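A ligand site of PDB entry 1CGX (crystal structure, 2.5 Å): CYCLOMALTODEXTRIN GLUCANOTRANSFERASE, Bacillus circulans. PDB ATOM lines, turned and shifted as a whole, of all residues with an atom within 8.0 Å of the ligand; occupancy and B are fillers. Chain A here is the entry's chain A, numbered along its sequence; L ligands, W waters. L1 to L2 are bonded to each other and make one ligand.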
ATOM      1  N   TYR A 301     -18.852   9.526 -18.903  1.00  0.00           N
ATOM      2  CA  TYR A 301     -19.671   9.768 -20.055  1.00  0.00           C
ATOM      3  C   TYR A 301     -20.754  10.747 -19.679  1.00  0.00           C
ATOM      4  O   TYR A 301     -21.238  11.525 -20.487  1.00  0.00           O
ATOM      5  CB  TYR A 301     -20.250   8.451 -20.576  1.00  0.00           C
ATOM      6  CG  TYR A 301     -19.143   7.577 -21.108  1.00  0.00           C
ATOM      7  CD1 TYR A 301     -18.626   7.882 -22.368  1.00  0.00           C
ATOM      8  CD2 TYR A 301     -18.524   6.579 -20.361  1.00  0.00           C
ATOM      9  CE1 TYR A 301     -17.566   7.168 -22.917  1.00  0.00           C
ATOM     10  CE2 TYR A 301     -17.459   5.848 -20.897  1.00  0.00           C
ATOM     11  CZ  TYR A 301     -16.995   6.123 -22.190  1.00  0.00           C
ATOM     12  OH  TYR A 301     -15.953   5.411 -22.731  1.00  0.00           O
ATOM     13  N   LYS A 304     -19.202  14.214 -19.320  1.00  0.00           N
ATOM     14  CA  LYS A 304     -18.974  14.751 -20.627  1.00  0.00           C
ATOM     15  C   LYS A 304     -20.270  15.214 -21.212  1.00  0.00           C
ATOM     16  O   LYS A 304     -20.361  16.241 -21.874  1.00  0.00           O
ATOM     17  CB  LYS A 304     -18.363  13.738 -21.557  1.00  0.00           C
ATOM     18  CG  LYS A 304     -18.512  14.176 -22.987  1.00  0.00           C
ATOM     19  CD  LYS A 304     -17.871  13.219 -23.982  1.00  0.00           C
ATOM     20  CE  LYS A 304     -18.542  13.214 -25.344  1.00  0.00           C
ATOM     21  NZ  LYS A 304     -17.612  13.060 -26.483  1.00  0.00           N
ATOM     22  N   GLN A 410     -13.032  20.647 -24.581  1.00  0.00           N
ATOM     23  CA  GLN A 410     -13.059  19.553 -25.510  1.00  0.00           C
ATOM     24  C   GLN A 410     -12.564  18.259 -24.946  1.00  0.00           C
ATOM     25  O   GLN A 410     -11.417  18.192 -24.502  1.00  0.00           O
ATOM     26  CB  GLN A 410     -12.198  19.887 -26.717  1.00  0.00           C
ATOM     27  CG  GLN A 410     -12.712  19.179 -27.967  1.00  0.00           C
ATOM     28  CD  GLN A 410     -11.693  19.150 -29.068  1.00  0.00           C
ATOM     29  OE1 GLN A 410     -11.799  18.310 -29.965  1.00  0.00           O
ATOM     30  NE2 GLN A 410     -10.717  19.992 -29.017  1.00  0.00           N
ATOM     31  N   GLU A 411     -13.413  17.228 -25.015  1.00  0.00           N
ATOM     32  CA  GLU A 411     -13.031  15.905 -24.557  1.00  0.00           C
ATOM     33  C   GLU A 411     -11.938  15.384 -25.488  1.00  0.00           C
ATOM     34  O   GLU A 411     -12.151  15.382 -26.699  1.00  0.00           O
ATOM     35  CB  GLU A 411     -14.248  14.945 -24.613  1.00  0.00           C
ATOM     36  CG  GLU A 411     -13.928  13.473 -24.292  1.00  0.00           C
ATOM     37  CD  GLU A 411     -13.637  12.687 -25.530  1.00  0.00           C
ATOM     38  OE1 GLU A 411     -14.430  12.519 -26.471  1.00  0.00           O
ATOM     39  OE2 GLU A 411     -12.486  12.165 -25.492  1.00  0.00           O
ATOM     40  N   ARG A 412     -10.781  14.926 -24.959  1.00  0.00           N
ATOM     41  CA  ARG A 412      -9.731  14.347 -25.828  1.00  0.00           C
ATOM     42  C   ARG A 412      -9.533  12.852 -25.588  1.00  0.00           C
ATOM     43  O   ARG A 412      -9.067  12.095 -26.438  1.00  0.00           O
ATOM     44  CB  ARG A 412      -8.370  15.022 -25.844  1.00  0.00           C
ATOM     45  CG  ARG A 412      -8.395  16.497 -25.602  1.00  0.00           C
ATOM     46  CD  ARG A 412      -8.497  17.403 -26.820  1.00  0.00           C
ATOM     47  NE  ARG A 412      -8.249  16.856 -28.132  1.00  0.00           N
ATOM     48  CZ  ARG A 412      -7.778  17.621 -29.163  1.00  0.00           C
ATOM     49  NH1 ARG A 412      -7.477  18.911 -29.057  1.00  0.00           N
ATOM     50  NH2 ARG A 412      -7.583  17.072 -30.354  1.00  0.00           N
ATOM     51  N   TRP A 413      -9.858  12.432 -24.388  1.00  0.00           N
ATOM     52  CA  TRP A 413      -9.740  11.056 -24.042  1.00  0.00           C
ATOM     53  C   TRP A 413     -10.783  10.735 -22.976  1.00  0.00           C
ATOM     54  O   TRP A 413     -11.043  11.523 -22.057  1.00  0.00           O
ATOM     55  CB  TRP A 413      -8.300  10.692 -23.642  1.00  0.00           C
ATOM     56  CG  TRP A 413      -7.855   9.283 -23.892  1.00  0.00           C
ATOM     57  CD1 TRP A 413      -7.081   8.871 -24.902  1.00  0.00           C
ATOM     58  CD2 TRP A 413      -8.055   8.154 -23.047  1.00  0.00           C
ATOM     59  NE1 TRP A 413      -6.815   7.541 -24.788  1.00  0.00           N
ATOM     60  CE2 TRP A 413      -7.399   7.071 -23.646  1.00  0.00           C
ATOM     61  CE3 TRP A 413      -8.763   7.957 -21.878  1.00  0.00           C
ATOM     62  CZ2 TRP A 413      -7.437   5.797 -23.094  1.00  0.00           C
ATOM     63  CZ3 TRP A 413      -8.814   6.701 -21.335  1.00  0.00           C
ATOM     64  CH2 TRP A 413      -8.149   5.627 -21.940  1.00  0.00           C
ATOM     65  N   ILE A 414     -11.381   9.556 -23.116  1.00  0.00           N
ATOM     66  CA  ILE A 414     -12.388   9.190 -22.149  1.00  0.00           C
ATOM     67  C   ILE A 414     -12.702   7.704 -22.011  1.00  0.00           C
ATOM     68  O   ILE A 414     -12.729   6.909 -22.939  1.00  0.00           O
ATOM     69  CB  ILE A 414     -13.697   9.943 -22.443  1.00  0.00           C
ATOM     70  CG1 ILE A 414     -14.780   9.564 -21.444  1.00  0.00           C
ATOM     71  CG2 ILE A 414     -14.200   9.639 -23.851  1.00  0.00           C
ATOM     72  CD1 ILE A 414     -15.981  10.473 -21.580  1.00  0.00           C
ATOM     73  N   ASN A 415     -13.045   7.339 -20.793  1.00  0.00           N
ATOM     74  CA  ASN A 415     -13.501   6.014 -20.459  1.00  0.00           C
ATOM     75  C   ASN A 415     -14.466   6.129 -19.269  1.00  0.00           C
ATOM     76  O   ASN A 415     -14.893   7.229 -18.936  1.00  0.00           O
ATOM     77  CB  ASN A 415     -12.446   4.899 -20.435  1.00  0.00           C
ATOM     78  CG  ASN A 415     -11.690   4.780 -19.121  1.00  0.00           C
ATOM     79  OD1 ASN A 415     -12.005   5.423 -18.123  1.00  0.00           O
ATOM     80  ND2 ASN A 415     -10.631   3.976 -19.134  1.00  0.00           N
ATOM     81  N   ASN A 416     -14.844   5.072 -18.617  1.00  0.00           N
ATOM     82  CA  ASN A 416     -15.771   5.246 -17.521  1.00  0.00           C
ATOM     83  C   ASN A 416     -15.300   6.117 -16.396  1.00  0.00           C
ATOM     84  O   ASN A 416     -16.095   6.829 -15.789  1.00  0.00           O
ATOM     85  CB  ASN A 416     -16.074   3.940 -16.797  1.00  0.00           C
ATOM     86  CG  ASN A 416     -16.902   2.975 -17.580  1.00  0.00           C
ATOM     87  OD1 ASN A 416     -17.019   1.829 -17.171  1.00  0.00           O
ATOM     88  ND2 ASN A 416     -17.445   3.435 -18.703  1.00  0.00           N
ATOM     89  N   VAL A 418     -12.054   7.808 -16.538  1.00  0.00           N
ATOM     90  CA  VAL A 418     -11.103   8.830 -16.869  1.00  0.00           C
ATOM     91  C   VAL A 418     -11.632   9.885 -17.806  1.00  0.00           C
ATOM     92  O   VAL A 418     -12.361   9.593 -18.749  1.00  0.00           O
ATOM     93  CB  VAL A 418      -9.907   8.208 -17.595  1.00  0.00           C
ATOM     94  CG1 VAL A 418      -8.950   9.268 -18.102  1.00  0.00           C
ATOM     95  CG2 VAL A 418      -9.192   7.161 -16.759  1.00  0.00           C
ATOM     96  N   LEU A 419     -11.167  11.085 -17.577  1.00  0.00           N
ATOM     97  CA  LEU A 419     -11.534  12.144 -18.462  1.00  0.00           C
ATOM     98  C   LEU A 419     -10.384  13.121 -18.701  1.00  0.00           C
ATOM     99  O   LEU A 419      -9.860  13.712 -17.786  1.00  0.00           O
ATOM    100  CB  LEU A 419     -12.802  12.874 -18.040  1.00  0.00           C
ATOM    101  CG  LEU A 419     -13.077  14.073 -18.952  1.00  0.00           C
ATOM    102  CD1 LEU A 419     -13.609  13.634 -20.320  1.00  0.00           C
ATOM    103  CD2 LEU A 419     -14.084  14.985 -18.274  1.00  0.00           C
ATOM    104  N   ILE A 420     -10.027  13.291 -19.957  1.00  0.00           N
ATOM    105  CA  ILE A 420      -9.004  14.226 -20.350  1.00  0.00           C
ATOM    106  C   ILE A 420      -9.617  15.283 -21.231  1.00  0.00           C
ATOM    107  O   ILE A 420     -10.138  14.994 -22.297  1.00  0.00           O
ATOM    108  CB  ILE A 420      -7.844  13.573 -21.072  1.00  0.00           C
ATOM    109  CG1 ILE A 420      -7.400  12.375 -20.250  1.00  0.00           C
ATOM    110  CG2 ILE A 420      -6.707  14.586 -21.209  1.00  0.00           C
ATOM    111  CD1 ILE A 420      -5.960  11.965 -20.557  1.00  0.00           C
ATOM    112  N   SER A 443      -4.203   3.102 -18.781  1.00  0.00           N
ATOM    113  CA  SER A 443      -3.229   3.170 -19.861  1.00  0.00           C
ATOM    114  C   SER A 443      -3.722   4.111 -20.880  1.00  0.00           C
ATOM    115  O   SER A 443      -4.682   3.829 -21.611  1.00  0.00           O
ATOM    116  CB  SER A 443      -2.970   1.853 -20.548  1.00  0.00           C
ATOM    117  OG  SER A 443      -1.677   1.432 -20.205  1.00  0.00           O
ATOM    118  N   ILE A 444      -3.063   5.225 -20.918  1.00  0.00           N
ATOM    119  CA  ILE A 444      -3.457   6.223 -21.842  1.00  0.00           C
ATOM    120  C   ILE A 444      -2.579   6.270 -23.040  1.00  0.00           C
ATOM    121  O   ILE A 444      -1.400   6.606 -22.917  1.00  0.00           O
ATOM    122  CB  ILE A 444      -3.623   7.553 -21.150  1.00  0.00           C
ATOM    123  CG1 ILE A 444      -4.931   7.479 -20.356  1.00  0.00           C
ATOM    124  CG2 ILE A 444      -3.671   8.653 -22.215  1.00  0.00           C
ATOM    125  CD1 ILE A 444      -4.843   8.086 -18.993  1.00  0.00           C
ATOM    126  N   SER A 445      -3.185   5.873 -24.160  1.00  0.00           N
ATOM    127  CA  SER A 445      -2.598   5.874 -25.482  1.00  0.00           C
ATOM    128  C   SER A 445      -3.641   6.482 -26.402  1.00  0.00           C
ATOM    129  O   SER A 445      -4.812   6.290 -26.160  1.00  0.00           O
ATOM    130  CB  SER A 445      -2.185   4.530 -26.081  1.00  0.00           C
ATOM    131  OG  SER A 445      -2.887   3.468 -25.512  1.00  0.00           O
ATOM    132  N   GLY A 446      -3.246   7.155 -27.427  1.00  0.00           N
ATOM    133  CA  GLY A 446      -3.933   7.866 -28.446  1.00  0.00           C
ATOM    134  C   GLY A 446      -4.341   9.274 -28.122  1.00  0.00           C
ATOM    135  O   GLY A 446      -5.193   9.855 -28.834  1.00  0.00           O
ATOM    136  N   LEU A 447      -3.761   9.821 -27.063  1.00  0.00           N
ATOM    137  CA  LEU A 447      -4.105  11.157 -26.662  1.00  0.00           C
ATOM    138  C   LEU A 447      -3.583  12.191 -27.651  1.00  0.00           C
ATOM    139  O   LEU A 447      -2.393  12.268 -27.942  1.00  0.00           O
ATOM    140  CB  LEU A 447      -3.636  11.441 -25.207  1.00  0.00           C
ATOM    141  CG  LEU A 447      -3.789  12.904 -24.766  1.00  0.00           C
ATOM    142  CD1 LEU A 447      -5.259  13.284 -24.691  1.00  0.00           C
ATOM    143  CD2 LEU A 447      -3.059  13.165 -23.456  1.00  0.00           C
ATOM    144  N   VAL A 448      -4.479  12.977 -28.207  1.00  0.00           N
ATOM    145  CA  VAL A 448      -4.024  13.993 -29.145  1.00  0.00           C
ATOM    146  C   VAL A 448      -4.379  15.356 -28.593  1.00  0.00           C
ATOM    147  O   VAL A 448      -5.493  15.544 -28.122  1.00  0.00           O
ATOM    148  CB  VAL A 448      -4.662  13.839 -30.520  1.00  0.00           C
ATOM    149  CG1 VAL A 448      -4.350  15.053 -31.364  1.00  0.00           C
ATOM    150  CG2 VAL A 448      -4.131  12.605 -31.222  1.00  0.00           C
ATOM    151  N   THR A 449      -3.464  16.306 -28.642  1.00  0.00           N
ATOM    152  CA  THR A 449      -3.811  17.615 -28.105  1.00  0.00           C
ATOM    153  C   THR A 449      -3.378  18.759 -28.983  1.00  0.00           C
ATOM    154  O   THR A 449      -2.741  18.589 -30.008  1.00  0.00           O
ATOM    155  CB  THR A 449      -3.137  17.847 -26.745  1.00  0.00           C
ATOM    156  OG1 THR A 449      -1.798  18.173 -26.995  1.00  0.00           O
ATOM    157  CG2 THR A 449      -3.136  16.547 -25.975  1.00  0.00           C
ATOM    158  N   ALA A 476       0.362  14.763 -30.731  1.00  0.00           N
ATOM    159  CA  ALA A 476       0.021  13.496 -30.136  1.00  0.00           C
ATOM    160  C   ALA A 476       0.929  13.187 -28.968  1.00  0.00           C
ATOM    161  O   ALA A 476       2.153  13.259 -29.078  1.00  0.00           O
ATOM    162  CB  ALA A 476       0.037  12.380 -31.153  1.00  0.00           C
HETATM  163  C1  LIG L   1      -9.490   4.836 -25.902  1.00  0.00           C
HETATM  164  C2  LIG L   1     -10.230   5.923 -25.202  1.00  0.00           C
HETATM  165  C3  LIG L   1     -10.724   6.928 -26.214  1.00  0.00           C
HETATM  166  C4  LIG L   1      -9.518   7.451 -26.979  1.00  0.00           C
HETATM  167  C5  LIG L   1      -8.831   6.291 -27.678  1.00  0.00           C
HETATM  168  C6  LIG L   1      -7.611   6.768 -28.427  1.00  0.00           C
HETATM  169  O1  LIG L   1     -10.389   4.206 -26.747  1.00  0.00           O
HETATM  170  O2  LIG L   1     -11.388   5.389 -24.564  1.00  0.00           O
HETATM  171  O3  LIG L   1     -11.356   7.984 -25.517  1.00  0.00           O
HETATM  172  O4  LIG L   1     -10.028   8.380 -27.963  1.00  0.00           O
HETATM  173  O5  LIG L   1      -8.396   5.408 -26.631  1.00  0.00           O
HETATM  174  O6  LIG L   1      -7.097   5.719 -29.249  1.00  0.00           O
HETATM  175  C1  LG2 L   2      -9.608   9.722 -27.945  1.00  0.00           C
HETATM  176  C2  LG2 L   2     -10.771  10.644 -28.233  1.00  0.00           C
HETATM  177  C3  LG2 L   2     -11.284  10.453 -29.642  1.00  0.00           C
HETATM  178  C4  LG2 L   2     -10.169  10.779 -30.609  1.00  0.00           C
HETATM  179  C5  LG2 L   2      -8.983   9.897 -30.286  1.00  0.00           C
HETATM  180  C6  LG2 L   2      -7.781  10.241 -31.106  1.00  0.00           C
HETATM  181  O1  LG2 L   2     -11.821  10.420 -27.315  1.00  0.00           O
HETATM  182  O2  LG2 L   2     -12.383  11.336 -29.883  1.00  0.00           O
HETATM  183  O3  LG2 L   2     -10.501  10.450 -31.962  1.00  0.00           O
HETATM  184  O4  LG2 L   2      -8.581   9.944 -28.908  1.00  0.00           O
HETATM  185  O5  LG2 L   2      -6.817   9.189 -31.074  1.00  0.00           O
HETATM  186  O   HOH W   1      -7.226  12.050 -28.251  1.00  0.00           O
HETATM  187  O   HOH W   2     -14.499   6.092 -24.876  1.00  0.00           O
HETATM  188  O   HOH W   3     -11.451  14.275 -29.092  1.00  0.00           O
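Water W3 bridges O of Glu 411 and O2 of LG2 L2.
Water W2 lies within hydrogen-bond range of the side-chain hydroxyl (OH) of Tyr 301 (2.7 Å), the backbone carbonyl oxygen (O) of Ile 414 (2.7 Å) and an oxygen (O2) of LIG L1 (3.2 Å).
N of Trp 413 sits at hydrogen-bond distance from OE2 of Glu 411.
OE1 of Glu 411 is in salt-bridge range of NZ of Lys 304, at 3.2 Å.
The guanidinium group (NE) of Arg 412 sits at hydrogen-bond distance from the backbone carbonyl oxygen (O) of Val 448, at 3.1 Å.
The backbone NH (N) of Arg 412 is in hydrogen-bond range of the backbone carbonyl oxygen (O) of Ile 420 (2.7 Å).
NH1 of Arg 412 sits close to NE2 of Gln 410 (3.4 Å).
O of Ser 445 lies within hydrogen-bond range of NE1 of Trp 413, at 2.7 Å.
The backbone carbonyl oxygen (O) of Trp 413 lies within hydrogen-bond range of the backbone NH (N) of Ile 420 (2.9 Å).
Merely in contact with the ligand: Ser 445 (3.6 Å).
Within 4 Å of the ligand: Glu 411, Arg 412, Trp 413, Ile 414, Ser 445 and Gly 446.
The nearest printed residue that does not touch the ligand is Asn 415 (4.3 Å).
The backbone NH of Ile 414 sits at hydrogen-bond distance from an oxygen (O3) of LIG L1 (2.9 Å).
The backbone carbonyl oxygen (O) of Ile 414 lies within hydrogen-bond range of an oxygen (O2) of LIG L1, at 2.6 Å.
The side-chain carboxylate (OE2) of Glu 411 is in hydrogen-bond range of an oxygen (O1) of LG2 L2, at 2.6 Å.
O of Gly 446 lies within hydrogen-bond range of O5 of LG2 L2.
The backbone carbonyl oxygen (O) of Arg 412 sits close to an oxygen (O1) of LG2 L2 (3.3 Å).
The indole nitrogen (NE1) of Trp 413 lies within hydrogen-bond range of an oxygen (O5) of LIG L1 (3.2 Å).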
